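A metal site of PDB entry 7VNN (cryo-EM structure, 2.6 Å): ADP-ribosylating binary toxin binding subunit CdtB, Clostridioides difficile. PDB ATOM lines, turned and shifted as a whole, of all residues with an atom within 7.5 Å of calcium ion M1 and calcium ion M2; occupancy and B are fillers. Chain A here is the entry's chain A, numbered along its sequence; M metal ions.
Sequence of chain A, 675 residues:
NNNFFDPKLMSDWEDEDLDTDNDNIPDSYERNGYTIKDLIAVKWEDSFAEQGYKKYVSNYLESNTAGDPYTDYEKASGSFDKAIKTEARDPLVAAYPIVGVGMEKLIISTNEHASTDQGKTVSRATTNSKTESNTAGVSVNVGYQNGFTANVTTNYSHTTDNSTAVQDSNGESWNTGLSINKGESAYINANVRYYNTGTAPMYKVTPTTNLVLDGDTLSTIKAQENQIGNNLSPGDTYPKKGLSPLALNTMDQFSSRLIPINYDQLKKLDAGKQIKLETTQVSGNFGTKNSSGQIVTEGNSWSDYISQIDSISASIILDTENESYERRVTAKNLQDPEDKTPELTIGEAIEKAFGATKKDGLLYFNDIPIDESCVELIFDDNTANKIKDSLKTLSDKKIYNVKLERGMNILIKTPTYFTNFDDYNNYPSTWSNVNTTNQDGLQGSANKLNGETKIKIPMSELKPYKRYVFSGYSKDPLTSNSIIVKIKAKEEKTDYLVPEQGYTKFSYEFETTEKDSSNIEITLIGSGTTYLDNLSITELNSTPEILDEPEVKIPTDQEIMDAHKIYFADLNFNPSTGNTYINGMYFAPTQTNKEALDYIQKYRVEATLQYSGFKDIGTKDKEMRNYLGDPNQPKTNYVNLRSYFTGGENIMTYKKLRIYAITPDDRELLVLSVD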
ATOM      1  N   LEU A  18     -20.605  19.994  13.671  1.00  0.00           N
ATOM      2  CA  LEU A  18     -21.456  18.945  13.124  1.00  0.00           C
ATOM      3  C   LEU A  18     -21.062  17.599  13.703  1.00  0.00           C
ATOM      4  O   LEU A  18     -19.884  17.252  13.770  1.00  0.00           O
ATOM      5  CB  LEU A  18     -21.344  18.923  11.595  1.00  0.00           C
ATOM      6  CG  LEU A  18     -22.452  18.154  10.864  1.00  0.00           C
ATOM      7  CD1 LEU A  18     -23.815  18.467  11.453  1.00  0.00           C
ATOM      8  CD2 LEU A  18     -22.416  18.478   9.378  1.00  0.00           C
ATOM      9  N   ASP A  19     -22.076  16.832  14.113  1.00  0.00           N
ATOM     10  CA  ASP A  19     -21.857  15.515  14.734  1.00  0.00           C
ATOM     11  C   ASP A  19     -23.021  14.628  14.321  1.00  0.00           C
ATOM     12  O   ASP A  19     -24.096  14.694  14.929  1.00  0.00           O
ATOM     13  CB  ASP A  19     -21.745  15.643  16.245  1.00  0.00           C
ATOM     14  CG  ASP A  19     -20.983  14.478  16.864  1.00  0.00           C
ATOM     15  OD1 ASP A  19     -20.687  13.506  16.150  1.00  0.00           O
ATOM     16  OD2 ASP A  19     -20.691  14.547  18.079  1.00  0.00           O
ATOM     17  N   THR A  20     -22.803  13.799  13.300  1.00  0.00           N
ATOM     18  CA  THR A  20     -23.883  12.989  12.742  1.00  0.00           C
ATOM     19  C   THR A  20     -24.123  11.692  13.498  1.00  0.00           C
ATOM     20  O   THR A  20     -25.272  11.310  13.702  1.00  0.00           O
ATOM     21  CB  THR A  20     -23.592  12.680  11.269  1.00  0.00           C
ATOM     22  OG1 THR A  20     -23.285  13.893  10.573  1.00  0.00           O
ATOM     23  CG2 THR A  20     -24.795  12.031  10.613  1.00  0.00           C
ATOM     24  N   ASP A  21     -23.056  11.004  13.924  1.00  0.00           N
ATOM     25  CA  ASP A  21     -23.201   9.765  14.658  1.00  0.00           C
ATOM     26  C   ASP A  21     -23.373   9.968  16.167  1.00  0.00           C
ATOM     27  O   ASP A  21     -23.647   8.998  16.870  1.00  0.00           O
ATOM     28  CB  ASP A  21     -21.994   8.854  14.409  1.00  0.00           C
ATOM     29  CG  ASP A  21     -20.675   9.571  14.611  1.00  0.00           C
ATOM     30  OD1 ASP A  21     -20.692  10.765  14.975  1.00  0.00           O
ATOM     31  OD2 ASP A  21     -19.615   8.951  14.396  1.00  0.00           O
ATOM     32  N   ASN A  22     -23.217  11.197  16.647  1.00  0.00           N
ATOM     33  CA  ASN A  22     -23.391  11.545  18.063  1.00  0.00           C
ATOM     34  C   ASN A  22     -22.444  10.738  18.949  1.00  0.00           C
ATOM     35  O   ASN A  22     -22.860  10.021  19.854  1.00  0.00           O
ATOM     36  CB  ASN A  22     -24.848  11.344  18.485  1.00  0.00           C
ATOM     37  CG  ASN A  22     -25.681  12.602  18.292  1.00  0.00           C
ATOM     38  OD1 ASN A  22     -25.417  13.401  17.400  1.00  0.00           O
ATOM     39  ND2 ASN A  22     -26.691  12.772  19.127  1.00  0.00           N
ATOM     40  N   ASP A  23     -21.139  10.880  18.682  1.00  0.00           N
ATOM     41  CA  ASP A  23     -20.100  10.335  19.547  1.00  0.00           C
ATOM     42  C   ASP A  23     -19.203  11.426  20.121  1.00  0.00           C
ATOM     43  O   ASP A  23     -18.049  11.169  20.460  1.00  0.00           O
ATOM     44  CB  ASP A  23     -19.273   9.294  18.790  1.00  0.00           C
ATOM     45  CG  ASP A  23     -18.617   9.848  17.551  1.00  0.00           C
ATOM     46  OD1 ASP A  23     -18.878  11.014  17.192  1.00  0.00           O
ATOM     47  OD2 ASP A  23     -17.821   9.118  16.922  1.00  0.00           O
ATOM     48  N   ASN A  24     -19.714  12.652  20.223  1.00  0.00           N
ATOM     49  CA  ASN A  24     -19.052  13.810  20.820  1.00  0.00           C
ATOM     50  C   ASN A  24     -17.825  14.272  20.042  1.00  0.00           C
ATOM     51  O   ASN A  24     -17.114  15.173  20.504  1.00  0.00           O
ATOM     52  CB  ASN A  24     -18.662  13.560  22.279  1.00  0.00           C
ATOM     53  CG  ASN A  24     -19.721  12.782  23.037  1.00  0.00           C
ATOM     54  OD1 ASN A  24     -20.906  13.086  22.961  1.00  0.00           O
ATOM     55  ND2 ASN A  24     -19.281  11.777  23.784  1.00  0.00           N
ATOM     56  N   ILE A  25     -17.554  13.688  18.877  1.00  0.00           N
ATOM     57  CA  ILE A  25     -16.439  14.092  18.031  1.00  0.00           C
ATOM     58  C   ILE A  25     -17.014  14.698  16.759  1.00  0.00           C
ATOM     59  O   ILE A  25     -17.820  14.047  16.088  1.00  0.00           O
ATOM     60  CB  ILE A  25     -15.504  12.923  17.684  1.00  0.00           C
ATOM     61  CG1 ILE A  25     -15.154  12.126  18.939  1.00  0.00           C
ATOM     62  CG2 ILE A  25     -14.229  13.436  17.026  1.00  0.00           C
ATOM     63  CD1 ILE A  25     -14.480  10.806  18.654  1.00  0.00           C
ATOM     64  N   PRO A  26     -16.658  15.929  16.400  1.00  0.00           N
ATOM     65  CA  PRO A  26     -17.175  16.518  15.160  1.00  0.00           C
ATOM     66  C   PRO A  26     -16.731  15.749  13.926  1.00  0.00           C
ATOM     67  O   PRO A  26     -15.690  15.091  13.924  1.00  0.00           O
ATOM     68  CB  PRO A  26     -16.595  17.939  15.174  1.00  0.00           C
ATOM     69  CG  PRO A  26     -16.332  18.215  16.613  1.00  0.00           C
ATOM     70  CD  PRO A  26     -15.930  16.913  17.215  1.00  0.00           C
ATOM     71  N   ASP A  27     -17.556  15.830  12.875  1.00  0.00           N
ATOM     72  CA  ASP A  27     -17.314  15.062  11.660  1.00  0.00           C
ATOM     73  C   ASP A  27     -16.003  15.459  10.996  1.00  0.00           C
ATOM     74  O   ASP A  27     -15.249  14.592  10.528  1.00  0.00           O
ATOM     75  CB  ASP A  27     -18.475  15.246  10.694  1.00  0.00           C
ATOM     76  CG  ASP A  27     -19.766  14.667  11.218  1.00  0.00           C
ATOM     77  OD1 ASP A  27     -19.762  14.116  12.345  1.00  0.00           O
ATOM     78  OD2 ASP A  27     -20.797  14.746  10.515  1.00  0.00           O
ATOM     79  N   SER A  28     -15.720  16.761  10.929  1.00  0.00           N
ATOM     80  CA  SER A  28     -14.492  17.213  10.267  1.00  0.00           C
ATOM     81  C   SER A  28     -13.260  16.718  11.008  1.00  0.00           C
ATOM     82  O   SER A  28     -12.240  16.404  10.387  1.00  0.00           O
ATOM     83  CB  SER A  28     -14.498  18.727  10.140  1.00  0.00           C
ATOM     84  OG  SER A  28     -14.766  19.350  11.387  1.00  0.00           O
ATOM     85  N   GLU A  30     -13.081  13.883  12.681  1.00  0.00           N
ATOM     86  CA  GLU A  30     -12.978  12.464  12.367  1.00  0.00           C
ATOM     87  C   GLU A  30     -12.409  12.260  10.970  1.00  0.00           C
ATOM     88  O   GLU A  30     -11.669  11.295  10.728  1.00  0.00           O
ATOM     89  CB  GLU A  30     -14.349  11.795  12.486  1.00  0.00           C
ATOM     90  CG  GLU A  30     -14.922  11.804  13.889  1.00  0.00           C
ATOM     91  CD  GLU A  30     -15.892  10.662  14.112  1.00  0.00           C
ATOM     92  OE1 GLU A  30     -15.468   9.494  14.049  1.00  0.00           O
ATOM     93  OE2 GLU A  30     -17.083  10.930  14.361  1.00  0.00           O
ATOM     94  N   TYR A  34      -7.615  13.849  14.717  1.00  0.00           N
ATOM     95  CA  TYR A  34      -7.865  14.538  15.984  1.00  0.00           C
ATOM     96  C   TYR A  34      -7.081  13.838  17.081  1.00  0.00           C
ATOM     97  O   TYR A  34      -6.398  12.842  16.854  1.00  0.00           O
ATOM     98  CB  TYR A  34      -9.362  14.556  16.302  1.00  0.00           C
ATOM     99  CG  TYR A  34      -9.983  13.193  16.464  1.00  0.00           C
ATOM    100  CD1 TYR A  34     -10.392  12.455  15.372  1.00  0.00           C
ATOM    101  CD2 TYR A  34     -10.156  12.628  17.731  1.00  0.00           C
ATOM    102  CE1 TYR A  34     -10.959  11.204  15.511  1.00  0.00           C
ATOM    103  CE2 TYR A  34     -10.714  11.380  17.890  1.00  0.00           C
ATOM    104  CZ  TYR A  34     -11.110  10.673  16.772  1.00  0.00           C
ATOM    105  OH  TYR A  34     -11.685   9.431  16.918  1.00  0.00           O
ATOM    106  N   SER A  58     -11.493   8.218  12.084  1.00  0.00           N
ATOM    107  CA  SER A  58     -12.573   7.256  12.284  1.00  0.00           C
ATOM    108  C   SER A  58     -13.732   7.598  11.359  1.00  0.00           C
ATOM    109  O   SER A  58     -13.791   8.673  10.769  1.00  0.00           O
ATOM    110  CB  SER A  58     -13.026   7.245  13.756  1.00  0.00           C
ATOM    111  OG  SER A  58     -13.243   8.561  14.227  1.00  0.00           O
ATOM    112  N   ASN A  59     -14.652   6.642  11.251  1.00  0.00           N
ATOM    113  CA  ASN A  59     -15.872   6.831  10.483  1.00  0.00           C
ATOM    114  C   ASN A  59     -16.770   7.831  11.179  1.00  0.00           C
ATOM    115  O   ASN A  59     -17.130   7.651  12.352  1.00  0.00           O
ATOM    116  CB  ASN A  59     -16.578   5.484  10.309  1.00  0.00           C
ATOM    117  CG  ASN A  59     -17.718   5.536   9.312  1.00  0.00           C
ATOM    118  OD1 ASN A  59     -18.206   6.605   8.956  1.00  0.00           O
ATOM    119  ND2 ASN A  59     -18.146   4.376   8.850  1.00  0.00           N
ATOM    120  N   TYR A  60     -17.152   8.893  10.471  1.00  0.00           N
ATOM    121  CA  TYR A  60     -17.975   9.949  11.040  1.00  0.00           C
ATOM    122  C   TYR A  60     -19.467   9.668  10.953  1.00  0.00           C
ATOM    123  O   TYR A  60     -20.263  10.432  11.506  1.00  0.00           O
ATOM    124  CB  TYR A  60     -17.662  11.299  10.372  1.00  0.00           C
ATOM    125  CG  TYR A  60     -18.160  11.417   8.944  1.00  0.00           C
ATOM    126  CD1 TYR A  60     -17.408  10.919   7.888  1.00  0.00           C
ATOM    127  CD2 TYR A  60     -19.359  12.049   8.664  1.00  0.00           C
ATOM    128  CE1 TYR A  60     -17.855  11.037   6.591  1.00  0.00           C
ATOM    129  CE2 TYR A  60     -19.814  12.165   7.360  1.00  0.00           C
ATOM    130  CZ  TYR A  60     -19.055  11.651   6.334  1.00  0.00           C
ATOM    131  OH  TYR A  60     -19.502  11.769   5.036  1.00  0.00           O
ATOM    132  N   LEU A  61     -19.866   8.597  10.265  1.00  0.00           N
ATOM    133  CA  LEU A  61     -21.267   8.191  10.189  1.00  0.00           C
ATOM    134  C   LEU A  61     -21.586   7.014  11.096  1.00  0.00           C
ATOM    135  O   LEU A  61     -22.728   6.567  11.121  1.00  0.00           O
ATOM    136  CB  LEU A  61     -21.657   7.858   8.746  1.00  0.00           C
ATOM    137  CG  LEU A  61     -21.787   9.031   7.774  1.00  0.00           C
ATOM    138  CD1 LEU A  61     -22.216   8.532   6.402  1.00  0.00           C
ATOM    139  CD2 LEU A  61     -22.766  10.052   8.305  1.00  0.00           C
ATOM    140  N   GLU A  62     -20.597   6.499  11.834  1.00  0.00           N
ATOM    141  CA  GLU A  62     -20.790   5.388  12.744  1.00  0.00           C
ATOM    142  C   GLU A  62     -20.132   5.695  14.078  1.00  0.00           C
ATOM    143  O   GLU A  62     -19.001   6.196  14.113  1.00  0.00           O
ATOM    144  CB  GLU A  62     -20.211   4.086  12.166  1.00  0.00           C
ATOM    145  CG  GLU A  62     -20.929   2.830  12.620  1.00  0.00           C
ATOM    146  CD  GLU A  62     -20.295   1.563  12.076  1.00  0.00           C
ATOM    147  OE1 GLU A  62     -19.550   1.652  11.075  1.00  0.00           O
ATOM    148  OE2 GLU A  62     -20.526   0.489  12.664  1.00  0.00           O
ATOM    149  N   SER A  63     -20.845   5.415  15.167  1.00  0.00           N
ATOM    150  CA  SER A  63     -20.282   5.609  16.493  1.00  0.00           C
ATOM    151  C   SER A  63     -19.299   4.523  16.897  1.00  0.00           C
ATOM    152  O   SER A  63     -18.472   4.745  17.782  1.00  0.00           O
ATOM    153  CB  SER A  63     -21.405   5.691  17.526  1.00  0.00           C
ATOM    154  OG  SER A  63     -20.888   5.956  18.821  1.00  0.00           O
ATOM    155  N   ASN A  64     -19.367   3.350  16.260  1.00  0.00           N
ATOM    156  CA  ASN A  64     -18.472   2.224  16.526  1.00  0.00           C
ATOM    157  C   ASN A  64     -17.792   1.864  15.207  1.00  0.00           C
ATOM    158  O   ASN A  64     -18.315   1.048  14.440  1.00  0.00           O
ATOM    159  CB  ASN A  64     -19.225   1.045  17.125  1.00  0.00           C
ATOM    160  CG  ASN A  64     -19.667   1.287  18.549  1.00  0.00           C
ATOM    161  OD1 ASN A  64     -18.983   0.932  19.491  1.00  0.00           O
ATOM    162  ND2 ASN A  64     -20.832   1.923  18.708  1.00  0.00           N
ATOM    163  N   THR A  65     -16.646   2.486  14.942  1.00  0.00           N
ATOM    164  CA  THR A  65     -15.953   2.247  13.681  1.00  0.00           C
ATOM    165  C   THR A  65     -15.451   0.805  13.581  1.00  0.00           C
ATOM    166  O   THR A  65     -15.578   0.169  12.530  1.00  0.00           O
ATOM    167  CB  THR A  65     -14.783   3.221  13.527  1.00  0.00           C
ATOM    168  OG1 THR A  65     -15.256   4.562  13.706  1.00  0.00           O
ATOM    169  CG2 THR A  65     -14.153   3.092  12.160  1.00  0.00           C
ATOM    170  N   THR A  71     -17.318   2.834  21.888  1.00  0.00           N
ATOM    171  CA  THR A  71     -17.453   3.859  20.875  1.00  0.00           C
ATOM    172  C   THR A  71     -16.090   4.490  20.553  1.00  0.00           C
ATOM    173  O   THR A  71     -15.088   4.250  21.233  1.00  0.00           O
ATOM    174  CB  THR A  71     -18.440   4.943  21.314  1.00  0.00           C
ATOM    175  OG1 THR A  71     -17.797   5.827  22.233  1.00  0.00           O
ATOM    176  CG2 THR A  71     -19.646   4.313  21.992  1.00  0.00           C
ATOM    177  N   ASP A  72     -16.082   5.315  19.497  1.00  0.00           N
ATOM    178  CA  ASP A  72     -14.839   5.932  19.052  1.00  0.00           C
ATOM    179  C   ASP A  72     -14.274   6.883  20.108  1.00  0.00           C
ATOM    180  O   ASP A  72     -13.067   6.876  20.380  1.00  0.00           O
ATOM    181  CB  ASP A  72     -15.068   6.667  17.735  1.00  0.00           C
ATOM    182  CG  ASP A  72     -15.369   5.722  16.596  1.00  0.00           C
ATOM    183  OD1 ASP A  72     -15.058   4.525  16.711  1.00  0.00           O
ATOM    184  OD2 ASP A  72     -15.925   6.188  15.573  1.00  0.00           O
ATOM    185  N   TYR A  73     -15.131   7.719  20.695  1.00  0.00           N
ATOM    186  CA  TYR A  73     -14.665   8.647  21.720  1.00  0.00           C
ATOM    187  C   TYR A  73     -14.168   7.900  22.956  1.00  0.00           C
ATOM    188  O   TYR A  73     -13.159   8.278  23.550  1.00  0.00           O
ATOM    189  CB  TYR A  73     -15.763   9.632  22.101  1.00  0.00           C
ATOM    190  CG  TYR A  73     -15.384  10.523  23.259  1.00  0.00           C
ATOM    191  CD1 TYR A  73     -14.517  11.588  23.089  1.00  0.00           C
ATOM    192  CD2 TYR A  73     -15.889  10.290  24.530  1.00  0.00           C
ATOM    193  CE1 TYR A  73     -14.164  12.403  24.143  1.00  0.00           C
ATOM    194  CE2 TYR A  73     -15.541  11.095  25.593  1.00  0.00           C
ATOM    195  CZ  TYR A  73     -14.683  12.154  25.389  1.00  0.00           C
ATOM    196  OH  TYR A  73     -14.328  12.960  26.444  1.00  0.00           O
ATOM    197  N   PRO A  91      -9.645   4.151  16.995  1.00  0.00           N
ATOM    198  CA  PRO A  91     -10.938   3.586  16.583  1.00  0.00           C
ATOM    199  C   PRO A  91     -10.837   2.514  15.512  1.00  0.00           C
ATOM    200  O   PRO A  91     -11.822   1.793  15.308  1.00  0.00           O
ATOM    201  CB  PRO A  91     -11.701   4.821  16.071  1.00  0.00           C
ATOM    202  CG  PRO A  91     -11.022   5.985  16.709  1.00  0.00           C
ATOM    203  CD  PRO A  91      -9.582   5.612  16.804  1.00  0.00           C
HETATM  204 CA    CA M   1     -17.410   7.955  14.732  1.00  0.00          CA
HETATM  205 CA    CA M   2     -18.899  12.245  15.054  1.00  0.00          CA
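The backbone carbonyl oxygen (O) of Glu 30 sits at hydrogen-bond distance from the backbone NH (N) of Ser 58 (3.4 Å). OG1 of Thr 65 lies within hydrogen-bond range of N of Asn 59 (3.3 Å). The backbone carbonyl oxygen (O) of Asp 19 sits close to the side-chain amide oxygen (OD1) of Asn 22, at 3.1 Å. The backbone NH (N) of Asn 24 sits at hydrogen-bond distance from the side-chain carboxylate (OD2) of Asp 19 (3.0 Å). The backbone NH (N) of Asp 72 lies within hydrogen-bond range of the backbone carbonyl oxygen (O) of Ser 63, at 3.0 Å. OD1 of Asp 72 sits at hydrogen-bond distance from OG1 of Thr 65 (3.0 Å). The side-chain carboxylate (OD2) of Asp 27 lies within hydrogen-bond range of the side-chain hydroxyl (OG1) of Thr 20, 2.6 Å away. The backbone carbonyl oxygen (O) of Leu 18 is in hydrogen-bond range of the backbone NH (N) of Asp 27 (2.9 Å).
Of the 25 residues printed, 6 come within 4 Å of calcium ion M1.
Merely in contact with calcium ion M2: Asp 27. Within 4 Å of calcium ion M2: Asp 19, Asp 21, Asp 23, Ile 25, Asp 27 and Glu 30.
Calcium ion M1 is bound by the backbone carbonyl oxygen of Asn 59 (2.4 Å), the side-chain carboxylate of Asp 21 (2.4 Å), the backbone carbonyl oxygen of Glu 62 (2.5 Å), the side-chain carboxylate of Asp 72 (2.5 Å), the side-chain carboxylate of Asp 23 (2.5 Å) and the side-chain carboxylate of Glu 30 (2.6 Å). Calcium ion M1 has six donor atoms within binding distance. Slightly farther from calcium ion M1 lies the side-chain carboxylate (OE2) of Glu 30 (3.0 Å).
Calcium ion M2 is bound by OD1 of Asp 21 (2.3 Å). O of Ile 25 is bound to calcium ion M2 (2.3 Å). The side-chain carboxylate (OE2) of Glu 30 binds calcium ion M2 (2.3 Å). Calcium ion M2 is bound by OD1 of Asp 19. The side-chain carboxylate (OD1) of Asp 23 is bound to calcium ion M2. Calcium ion M2 has five donor atoms within binding distance.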
